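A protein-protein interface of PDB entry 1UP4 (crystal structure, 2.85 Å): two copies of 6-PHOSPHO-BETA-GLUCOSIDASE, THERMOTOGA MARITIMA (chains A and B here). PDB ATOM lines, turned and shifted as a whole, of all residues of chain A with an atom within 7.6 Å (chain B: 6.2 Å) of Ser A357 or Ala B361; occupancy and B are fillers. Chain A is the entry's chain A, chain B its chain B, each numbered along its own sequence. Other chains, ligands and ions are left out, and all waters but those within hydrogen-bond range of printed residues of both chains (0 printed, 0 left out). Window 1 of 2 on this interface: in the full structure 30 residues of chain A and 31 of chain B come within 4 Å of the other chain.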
ATOM      1  N   LEU A 193     -13.144  38.437  -3.432  1.00  0.00           N
ATOM      2  CA  LEU A 193     -12.677  37.295  -2.695  1.00  0.00           C
ATOM      3  C   LEU A 193     -12.570  37.756  -1.254  1.00  0.00           C
ATOM      4  O   LEU A 193     -11.526  37.682  -0.641  1.00  0.00           O
ATOM      5  CB  LEU A 193     -11.320  36.889  -3.222  1.00  0.00           C
ATOM      6  CG  LEU A 193     -10.975  35.430  -3.500  1.00  0.00           C
ATOM      7  CD1 LEU A 193      -9.760  35.114  -2.668  1.00  0.00           C
ATOM      8  CD2 LEU A 193     -12.094  34.439  -3.270  1.00  0.00           C
ATOM      9  N   PHE A 195     -14.339  38.702   2.851  1.00  0.00           N
ATOM     10  CA  PHE A 195     -14.949  38.048   4.005  1.00  0.00           C
ATOM     11  C   PHE A 195     -15.283  39.102   5.040  1.00  0.00           C
ATOM     12  O   PHE A 195     -14.507  40.035   5.245  1.00  0.00           O
ATOM     13  CB  PHE A 195     -13.974  37.011   4.593  1.00  0.00           C
ATOM     14  CG  PHE A 195     -13.478  35.993   3.577  1.00  0.00           C
ATOM     15  CD1 PHE A 195     -12.446  36.318   2.686  1.00  0.00           C
ATOM     16  CD2 PHE A 195     -14.066  34.732   3.506  1.00  0.00           C
ATOM     17  CE1 PHE A 195     -12.000  35.394   1.729  1.00  0.00           C
ATOM     18  CE2 PHE A 195     -13.640  33.802   2.572  1.00  0.00           C
ATOM     19  CZ  PHE A 195     -12.596  34.121   1.671  1.00  0.00           C
ATOM     20  N   LEU A 326      -1.111  38.710   7.686  1.00  0.00           N
ATOM     21  CA  LEU A 326      -0.842  38.703   6.254  1.00  0.00           C
ATOM     22  C   LEU A 326       0.306  39.680   5.942  1.00  0.00           C
ATOM     23  O   LEU A 326       0.480  40.690   6.630  1.00  0.00           O
ATOM     24  CB  LEU A 326      -2.115  39.116   5.520  1.00  0.00           C
ATOM     25  CG  LEU A 326      -2.916  38.152   4.626  1.00  0.00           C
ATOM     26  CD1 LEU A 326      -2.783  36.748   5.074  1.00  0.00           C
ATOM     27  CD2 LEU A 326      -4.400  38.484   4.519  1.00  0.00           C
ATOM     28  N   ASP A 352      -9.014  35.031   9.523  1.00  0.00           N
ATOM     29  CA  ASP A 352      -9.391  33.634   9.656  1.00  0.00           C
ATOM     30  C   ASP A 352      -8.558  32.716   8.745  1.00  0.00           C
ATOM     31  O   ASP A 352      -8.342  33.058   7.575  1.00  0.00           O
ATOM     32  CB  ASP A 352     -10.864  33.513   9.277  1.00  0.00           C
ATOM     33  CG  ASP A 352     -11.483  32.229   9.770  1.00  0.00           C
ATOM     34  OD1 ASP A 352     -11.157  31.146   9.213  1.00  0.00           O
ATOM     35  OD2 ASP A 352     -12.295  32.211  10.726  1.00  0.00           O
ATOM     36  N   HIS A 353      -8.124  31.546   9.240  1.00  0.00           N
ATOM     37  CA  HIS A 353      -7.355  30.621   8.369  1.00  0.00           C
ATOM     38  C   HIS A 353      -8.078  30.248   7.086  1.00  0.00           C
ATOM     39  O   HIS A 353      -7.459  30.075   6.052  1.00  0.00           O
ATOM     40  CB  HIS A 353      -6.940  29.335   9.061  1.00  0.00           C
ATOM     41  CG  HIS A 353      -6.146  29.555  10.297  1.00  0.00           C
ATOM     42  ND1 HIS A 353      -6.260  28.743  11.403  1.00  0.00           N
ATOM     43  CD2 HIS A 353      -5.250  30.515  10.619  1.00  0.00           C
ATOM     44  CE1 HIS A 353      -5.458  29.188  12.351  1.00  0.00           C
ATOM     45  NE2 HIS A 353      -4.835  30.263  11.901  1.00  0.00           N
ATOM     46  N   PHE A 354      -9.393  30.127   7.173  1.00  0.00           N
ATOM     47  CA  PHE A 354     -10.224  29.769   6.049  1.00  0.00           C
ATOM     48  C   PHE A 354     -10.063  30.813   4.957  1.00  0.00           C
ATOM     49  O   PHE A 354      -9.805  30.466   3.795  1.00  0.00           O
ATOM     50  CB  PHE A 354     -11.686  29.672   6.501  1.00  0.00           C
ATOM     51  CG  PHE A 354     -12.633  29.209   5.431  1.00  0.00           C
ATOM     52  CD1 PHE A 354     -12.853  27.854   5.219  1.00  0.00           C
ATOM     53  CD2 PHE A 354     -13.307  30.130   4.637  1.00  0.00           C
ATOM     54  CE1 PHE A 354     -13.726  27.428   4.228  1.00  0.00           C
ATOM     55  CE2 PHE A 354     -14.174  29.715   3.656  1.00  0.00           C
ATOM     56  CZ  PHE A 354     -14.387  28.350   3.450  1.00  0.00           C
ATOM     57  N   ALA A 355     -10.200  32.089   5.342  1.00  0.00           N
ATOM     58  CA  ALA A 355     -10.122  33.208   4.402  1.00  0.00           C
ATOM     59  C   ALA A 355      -8.723  33.320   3.822  1.00  0.00           C
ATOM     60  O   ALA A 355      -8.543  33.536   2.614  1.00  0.00           O
ATOM     61  CB  ALA A 355     -10.492  34.490   5.079  1.00  0.00           C
ATOM     62  N   LEU A 356      -7.730  33.141   4.687  1.00  0.00           N
ATOM     63  CA  LEU A 356      -6.335  33.231   4.294  1.00  0.00           C
ATOM     64  C   LEU A 356      -5.959  32.174   3.245  1.00  0.00           C
ATOM     65  O   LEU A 356      -5.142  32.463   2.347  1.00  0.00           O
ATOM     66  CB  LEU A 356      -5.441  33.153   5.529  1.00  0.00           C
ATOM     67  CG  LEU A 356      -5.018  34.503   6.123  1.00  0.00           C
ATOM     68  CD1 LEU A 356      -6.182  35.374   6.623  1.00  0.00           C
ATOM     69  CD2 LEU A 356      -4.002  34.262   7.253  1.00  0.00           C
ATOM     70  N   SER A 357      -6.558  30.979   3.319  1.00  0.00           N
ATOM     71  CA  SER A 357      -6.240  29.957   2.320  1.00  0.00           C
ATOM     72  C   SER A 357      -6.564  30.483   0.949  1.00  0.00           C
ATOM     73  O   SER A 357      -5.763  30.302   0.061  1.00  0.00           O
ATOM     74  CB  SER A 357      -6.969  28.637   2.550  1.00  0.00           C
ATOM     75  OG  SER A 357      -8.361  28.771   2.260  1.00  0.00           O
ATOM     76  N   PHE A 358      -7.711  31.151   0.775  1.00  0.00           N
ATOM     77  CA  PHE A 358      -8.052  31.718  -0.527  1.00  0.00           C
ATOM     78  C   PHE A 358      -7.179  32.928  -0.837  1.00  0.00           C
ATOM     79  O   PHE A 358      -6.610  33.010  -1.929  1.00  0.00           O
ATOM     80  CB  PHE A 358      -9.500  32.128  -0.589  1.00  0.00           C
ATOM     81  CG  PHE A 358     -10.432  31.017  -0.483  1.00  0.00           C
ATOM     82  CD1 PHE A 358     -10.764  30.278  -1.615  1.00  0.00           C
ATOM     83  CD2 PHE A 358     -11.011  30.694   0.744  1.00  0.00           C
ATOM     84  CE1 PHE A 358     -11.630  29.226  -1.519  1.00  0.00           C
ATOM     85  CE2 PHE A 358     -11.900  29.625   0.849  1.00  0.00           C
ATOM     86  CZ  PHE A 358     -12.211  28.903  -0.269  1.00  0.00           C
ATOM     87  N   ILE A 359      -7.079  33.861   0.119  1.00  0.00           N
ATOM     88  CA  ILE A 359      -6.266  35.073  -0.059  1.00  0.00           C
ATOM     89  C   ILE A 359      -4.840  34.767  -0.537  1.00  0.00           C
ATOM     90  O   ILE A 359      -4.427  35.301  -1.565  1.00  0.00           O
ATOM     91  CB  ILE A 359      -6.265  35.937   1.222  1.00  0.00           C
ATOM     92  CG1 ILE A 359      -7.686  36.410   1.581  1.00  0.00           C
ATOM     93  CG2 ILE A 359      -5.376  37.142   1.057  1.00  0.00           C
ATOM     94  CD1 ILE A 359      -7.855  36.771   3.100  1.00  0.00           C
ATOM     95  N   HIS A 360      -4.121  33.888   0.174  1.00  0.00           N
ATOM     96  CA  HIS A 360      -2.768  33.474  -0.214  1.00  0.00           C
ATOM     97  C   HIS A 360      -2.721  32.817  -1.606  1.00  0.00           C
ATOM     98  O   HIS A 360      -1.903  33.162  -2.455  1.00  0.00           O
ATOM     99  CB  HIS A 360      -2.200  32.477   0.794  1.00  0.00           C
ATOM    100  CG  HIS A 360      -1.625  33.086   2.040  1.00  0.00           C
ATOM    101  ND1 HIS A 360      -0.576  33.982   2.027  1.00  0.00           N
ATOM    102  CD2 HIS A 360      -1.918  32.869   3.346  1.00  0.00           C
ATOM    103  CE1 HIS A 360      -0.265  34.308   3.271  1.00  0.00           C
ATOM    104  NE2 HIS A 360      -1.064  33.647   4.090  1.00  0.00           N
ATOM    105  N   ALA A 361      -3.595  31.854  -1.839  1.00  0.00           N
ATOM    106  CA  ALA A 361      -3.599  31.174  -3.142  1.00  0.00           C
ATOM    107  C   ALA A 361      -3.708  32.154  -4.340  1.00  0.00           C
ATOM    108  O   ALA A 361      -2.913  32.097  -5.301  1.00  0.00           O
ATOM    109  CB  ALA A 361      -4.709  30.153  -3.202  1.00  0.00           C
ATOM    110  N   VAL A 362      -4.695  33.037  -4.283  1.00  0.00           N
ATOM    111  CA  VAL A 362      -4.974  33.914  -5.394  1.00  0.00           C
ATOM    112  C   VAL A 362      -3.934  35.043  -5.482  1.00  0.00           C
ATOM    113  O   VAL A 362      -3.605  35.528  -6.587  1.00  0.00           O
ATOM    114  CB  VAL A 362      -6.444  34.447  -5.318  1.00  0.00           C
ATOM    115  CG1 VAL A 362      -6.743  35.533  -6.372  1.00  0.00           C
ATOM    116  CG2 VAL A 362      -7.423  33.272  -5.404  1.00  0.00           C
ATOM    117  N   LYS A 363      -3.403  35.450  -4.339  1.00  0.00           N
ATOM    118  CA  LYS A 363      -2.368  36.457  -4.362  1.00  0.00           C
ATOM    119  C   LYS A 363      -1.133  35.961  -5.102  1.00  0.00           C
ATOM    120  O   LYS A 363      -0.566  36.708  -5.890  1.00  0.00           O
ATOM    121  CB  LYS A 363      -1.977  36.910  -2.959  1.00  0.00           C
ATOM    122  CG  LYS A 363      -1.061  38.161  -2.982  1.00  0.00           C
ATOM    123  CD  LYS A 363      -1.689  39.296  -3.804  1.00  0.00           C
ATOM    124  CE  LYS A 363      -2.738  40.063  -2.992  1.00  0.00           C
ATOM    125  NZ  LYS A 363      -3.173  41.262  -3.706  1.00  0.00           N
ATOM    126  N   PRO A 389      -6.501  28.493  -8.324  1.00  0.00           N
ATOM    127  CA  PRO A 389      -7.396  27.450  -7.786  1.00  0.00           C
ATOM    128  C   PRO A 389      -8.482  27.014  -8.744  1.00  0.00           C
ATOM    129  O   PRO A 389      -8.928  25.891  -8.667  1.00  0.00           O
ATOM    130  CB  PRO A 389      -8.030  28.129  -6.583  1.00  0.00           C
ATOM    131  CG  PRO A 389      -6.968  29.048  -6.115  1.00  0.00           C
ATOM    132  CD  PRO A 389      -6.396  29.628  -7.395  1.00  0.00           C
ATOM    133  N   LEU B 356       4.594  28.374  -3.122  1.00  0.00           N
ATOM    134  CA  LEU B 356       3.966  28.985  -1.951  1.00  0.00           C
ATOM    135  C   LEU B 356       2.443  28.897  -2.042  1.00  0.00           C
ATOM    136  O   LEU B 356       1.767  28.743  -1.011  1.00  0.00           O
ATOM    137  CB  LEU B 356       4.430  30.429  -1.759  1.00  0.00           C
ATOM    138  CG  LEU B 356       5.585  30.712  -0.784  1.00  0.00           C
ATOM    139  CD1 LEU B 356       6.859  29.796  -0.890  1.00  0.00           C
ATOM    140  CD2 LEU B 356       5.994  32.184  -0.860  1.00  0.00           C
ATOM    141  N   SER B 357       1.885  28.955  -3.251  1.00  0.00           N
ATOM    142  CA  SER B 357       0.432  28.875  -3.335  1.00  0.00           C
ATOM    143  C   SER B 357      -0.048  27.555  -2.756  1.00  0.00           C
ATOM    144  O   SER B 357      -1.006  27.531  -1.990  1.00  0.00           O
ATOM    145  CB  SER B 357      -0.121  29.132  -4.735  1.00  0.00           C
ATOM    146  OG  SER B 357       0.102  28.039  -5.586  1.00  0.00           O
ATOM    147  N   PHE B 358       0.642  26.462  -3.066  1.00  0.00           N
ATOM    148  CA  PHE B 358       0.282  25.185  -2.452  1.00  0.00           C
ATOM    149  C   PHE B 358       0.591  25.179  -0.961  1.00  0.00           C
ATOM    150  O   PHE B 358      -0.278  24.814  -0.156  1.00  0.00           O
ATOM    151  CB  PHE B 358       0.967  24.032  -3.141  1.00  0.00           C
ATOM    152  CG  PHE B 358       0.531  23.839  -4.522  1.00  0.00           C
ATOM    153  CD1 PHE B 358      -0.672  23.188  -4.790  1.00  0.00           C
ATOM    154  CD2 PHE B 358       1.322  24.299  -5.585  1.00  0.00           C
ATOM    155  CE1 PHE B 358      -1.080  22.991  -6.084  1.00  0.00           C
ATOM    156  CE2 PHE B 358       0.916  24.103  -6.916  1.00  0.00           C
ATOM    157  CZ  PHE B 358      -0.291  23.449  -7.172  1.00  0.00           C
ATOM    158  N   ILE B 359       1.806  25.588  -0.588  1.00  0.00           N
ATOM    159  CA  ILE B 359       2.196  25.561   0.818  1.00  0.00           C
ATOM    160  C   ILE B 359       1.223  26.334   1.741  1.00  0.00           C
ATOM    161  O   ILE B 359       0.763  25.780   2.747  1.00  0.00           O
ATOM    162  CB  ILE B 359       3.636  26.030   1.007  1.00  0.00           C
ATOM    163  CG1 ILE B 359       4.593  25.048   0.330  1.00  0.00           C
ATOM    164  CG2 ILE B 359       3.951  26.171   2.480  1.00  0.00           C
ATOM    165  CD1 ILE B 359       5.819  25.725  -0.249  1.00  0.00           C
ATOM    166  N   HIS B 360       0.879  27.569   1.378  1.00  0.00           N
ATOM    167  CA  HIS B 360      -0.082  28.365   2.138  1.00  0.00           C
ATOM    168  C   HIS B 360      -1.472  27.721   2.224  1.00  0.00           C
ATOM    169  O   HIS B 360      -2.081  27.644   3.276  1.00  0.00           O
ATOM    170  CB  HIS B 360      -0.259  29.736   1.494  1.00  0.00           C
ATOM    171  CG  HIS B 360       0.795  30.730   1.854  1.00  0.00           C
ATOM    172  ND1 HIS B 360       1.046  31.114   3.156  1.00  0.00           N
ATOM    173  CD2 HIS B 360       1.640  31.450   1.073  1.00  0.00           C
ATOM    174  CE1 HIS B 360       2.007  32.024   3.158  1.00  0.00           C
ATOM    175  NE2 HIS B 360       2.387  32.240   1.909  1.00  0.00           N
ATOM    176  N   ALA B 361      -1.986  27.278   1.089  1.00  0.00           N
ATOM    177  CA  ALA B 361      -3.348  26.746   1.048  1.00  0.00           C
ATOM    178  C   ALA B 361      -3.531  25.590   2.036  1.00  0.00           C
ATOM    179  O   ALA B 361      -4.467  25.593   2.847  1.00  0.00           O
ATOM    180  CB  ALA B 361      -3.693  26.294  -0.364  1.00  0.00           C
ATOM    181  N   VAL B 362      -2.642  24.585   1.954  1.00  0.00           N
ATOM    182  CA  VAL B 362      -2.839  23.389   2.775  1.00  0.00           C
ATOM    183  C   VAL B 362      -2.330  23.550   4.207  1.00  0.00           C
ATOM    184  O   VAL B 362      -2.735  22.824   5.112  1.00  0.00           O
ATOM    185  CB  VAL B 362      -2.304  22.105   2.072  1.00  0.00           C
ATOM    186  CG1 VAL B 362      -1.803  22.435   0.690  1.00  0.00           C
ATOM    187  CG2 VAL B 362      -1.210  21.448   2.894  1.00  0.00           C
ATOM    188  N   LYS B 363      -1.409  24.497   4.406  1.00  0.00           N
ATOM    189  CA  LYS B 363      -1.067  24.866   5.768  1.00  0.00           C
ATOM    190  C   LYS B 363      -2.282  25.444   6.507  1.00  0.00           C
ATOM    191  O   LYS B 363      -2.510  25.142   7.666  1.00  0.00           O
ATOM    192  CB  LYS B 363       0.079  25.873   5.776  1.00  0.00           C
ATOM    193  CG  LYS B 363       0.438  26.306   7.204  1.00  0.00           C
ATOM    194  CD  LYS B 363       1.743  25.706   7.699  1.00  0.00           C
ATOM    195  CE  LYS B 363       1.624  24.226   8.018  1.00  0.00           C
ATOM    196  NZ  LYS B 363       2.925  23.548   7.900  1.00  0.00           N
ATOM    197  N   MET B 364      -3.095  26.238   5.820  1.00  0.00           N
ATOM    198  CA  MET B 364      -4.309  26.774   6.419  1.00  0.00           C
ATOM    199  C   MET B 364      -5.272  25.622   6.716  1.00  0.00           C
ATOM    200  O   MET B 364      -5.844  25.534   7.821  1.00  0.00           O
ATOM    201  CB  MET B 364      -4.951  27.840   5.545  1.00  0.00           C
ATOM    202  CG  MET B 364      -4.145  29.099   5.365  1.00  0.00           C
ATOM    203  SD  MET B 364      -3.561  30.040   7.013  1.00  0.00           S
ATOM    204  CE  MET B 364      -1.834  29.020   7.411  1.00  0.00           C
ATOM    205  N   TYR B 365      -5.407  24.722   5.745  1.00  0.00           N
ATOM    206  CA  TYR B 365      -6.201  23.516   5.919  1.00  0.00           C
ATOM    207  C   TYR B 365      -5.678  22.692   7.136  1.00  0.00           C
ATOM    208  O   TYR B 365      -6.457  22.166   7.935  1.00  0.00           O
ATOM    209  CB  TYR B 365      -6.250  22.660   4.612  1.00  0.00           C
ATOM    210  CG  TYR B 365      -6.281  21.182   4.929  1.00  0.00           C
ATOM    211  CD1 TYR B 365      -5.097  20.476   5.123  1.00  0.00           C
ATOM    212  CD2 TYR B 365      -7.491  20.510   5.127  1.00  0.00           C
ATOM    213  CE1 TYR B 365      -5.109  19.152   5.484  1.00  0.00           C
ATOM    214  CE2 TYR B 365      -7.510  19.162   5.501  1.00  0.00           C
ATOM    215  CZ  TYR B 365      -6.309  18.492   5.683  1.00  0.00           C
ATOM    216  OH  TYR B 365      -6.278  17.147   6.037  1.00  0.00           O
ATOM    217  N   GLU B 366      -4.360  22.584   7.262  1.00  0.00           N
ATOM    218  CA  GLU B 366      -3.754  21.818   8.346  1.00  0.00           C
ATOM    219  C   GLU B 366      -4.163  22.347   9.709  1.00  0.00           C
ATOM    220  O   GLU B 366      -4.548  21.568  10.594  1.00  0.00           O
ATOM    221  CB  GLU B 366      -2.223  21.796   8.239  1.00  0.00           C
ATOM    222  CG  GLU B 366      -1.673  20.710   7.342  1.00  0.00           C
ATOM    223  CD  GLU B 366      -0.138  20.667   7.283  1.00  0.00           C
ATOM    224  OE1 GLU B 366       0.549  21.618   7.755  1.00  0.00           O
ATOM    225  OE2 GLU B 366       0.405  19.644   6.763  1.00  0.00           O
ATOM    226  N   LEU B 368      -6.696  24.490  10.342  1.00  0.00           N
ATOM    227  CA  LEU B 368      -8.152  24.423  10.511  1.00  0.00           C
ATOM    228  C   LEU B 368      -8.552  23.056  11.015  1.00  0.00           C
ATOM    229  O   LEU B 368      -9.442  22.954  11.840  1.00  0.00           O
ATOM    230  CB  LEU B 368      -8.905  24.748   9.217  1.00  0.00           C
ATOM    231  CG  LEU B 368      -8.930  26.209   8.795  1.00  0.00           C
ATOM    232  CD1 LEU B 368      -9.290  26.373   7.336  1.00  0.00           C
ATOM    233  CD2 LEU B 368      -9.854  26.969   9.613  1.00  0.00           C
ATOM    234  N   SER B 387     -11.774  23.794   3.139  1.00  0.00           N
ATOM    235  CA  SER B 387     -10.618  24.605   2.842  1.00  0.00           C
ATOM    236  C   SER B 387      -9.529  23.886   2.045  1.00  0.00           C
ATOM    237  O   SER B 387      -8.601  24.532   1.533  1.00  0.00           O
ATOM    238  CB  SER B 387     -10.048  25.132   4.146  1.00  0.00           C
ATOM    239  OG  SER B 387      -9.317  24.098   4.797  1.00  0.00           O
ATOM    240  N   HIS B 388      -9.623  22.559   1.944  1.00  0.00           N
ATOM    241  CA  HIS B 388      -8.616  21.796   1.221  1.00  0.00           C
ATOM    242  C   HIS B 388      -8.769  21.941  -0.290  1.00  0.00           C
ATOM    243  O   HIS B 388      -9.869  21.753  -0.832  1.00  0.00           O
ATOM    244  CB  HIS B 388      -8.661  20.314   1.619  1.00  0.00           C
ATOM    245  CG  HIS B 388      -7.367  19.593   1.346  1.00  0.00           C
ATOM    246  ND1 HIS B 388      -6.801  19.519   0.086  1.00  0.00           N
ATOM    247  CD2 HIS B 388      -6.503  18.963   2.181  1.00  0.00           C
ATOM    248  CE1 HIS B 388      -5.653  18.865   0.155  1.00  0.00           C
ATOM    249  NE2 HIS B 388      -5.448  18.515   1.412  1.00  0.00           N
ATOM    250  N   PRO B 389      -7.690  22.290  -0.993  1.00  0.00           N
ATOM    251  CA  PRO B 389      -7.750  22.388  -2.459  1.00  0.00           C
ATOM    252  C   PRO B 389      -8.379  21.144  -3.113  1.00  0.00           C
ATOM    253  O   PRO B 389      -8.974  21.248  -4.177  1.00  0.00           O
ATOM    254  CB  PRO B 389      -6.295  22.559  -2.855  1.00  0.00           C
ATOM    255  CG  PRO B 389      -5.701  23.210  -1.728  1.00  0.00           C
ATOM    256  CD  PRO B 389      -6.365  22.666  -0.482  1.00  0.00           C
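A ring nitrogen (NE2) of His A360 sits at hydrogen-bond distance from a ring nitrogen (ND1) of His B360.
The backbone NH (N) of Phe A354 is in hydrogen-bond range of the side-chain carboxylate (OD1) of Asp A352, at 2.9 Å.
The backbone carbonyl oxygen (O) of Phe A354 is in hydrogen-bond range of the side-chain hydroxyl (OG) of Ser A357, 2.7 Å away.
Among the printed residues, merely in contact across the chains: His A353 with Met B364, Ser A357 with Met B364, His A353 with Leu B368, Phe A354 with Leu B368, Leu A356 with Met B364 and Ser A357 with Ala B361.
Printed residues of chain B within 4 Å of His A353: Met B364 and Leu B368.
Of the printed residues of chain B, Leu A356 touches Met B364.
Lys A363 touches none of the printed residues of chain B.
Printed residues of chain A within 4 Å of Ala B361: Ser A357.
Printed residues of chain A within 4 Å of Met B364: His A353 (3.4 Å), Leu A356 (3.9 Å) and Ser A357 (3.7 Å).
Printed residues of chain A within 4 Å of Leu B368: His A353 (3.7 Å) and Phe A354 (3.7 Å).
The nearest residue of chain B that does not touch Ser A357 is Ser B387 (4.3 Å).
The nearest residue of chain A that does not touch Ala B361 is Ala A361 (4.9 Å).
The nearest printed residue of chain B that does not touch His A360 is Met B364 (4.8 Å).
Of the 16 printed residues of chain A, 5 touch a printed residue of chain B.
Hydrophobic or aromatic side chains of chain A within 4 Å of the printed part of chain B: His A353, Leu A356 and His A360.
Hydrophobic or aromatic side chains of chain B that line the printed part of chain A: His B360, Met B364 and Leu B368.
Among the printed residues, 7 pairs touch across the chains.
Among the printed residues, no Asp or Glu carboxylate lies within 4 Å of a Lys or Arg side-chain nitrogen of the other chain.
Ser A357 touches Ala B361, but with the chains exchanged Ala A361 does not touch Ser B357 (4.1 Å).
His B360 touches its own counterpart, His A360.
Of the 7 pairs that touch across the chains among the printed residues, 1 has its exchanged pair printed and touching as well.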
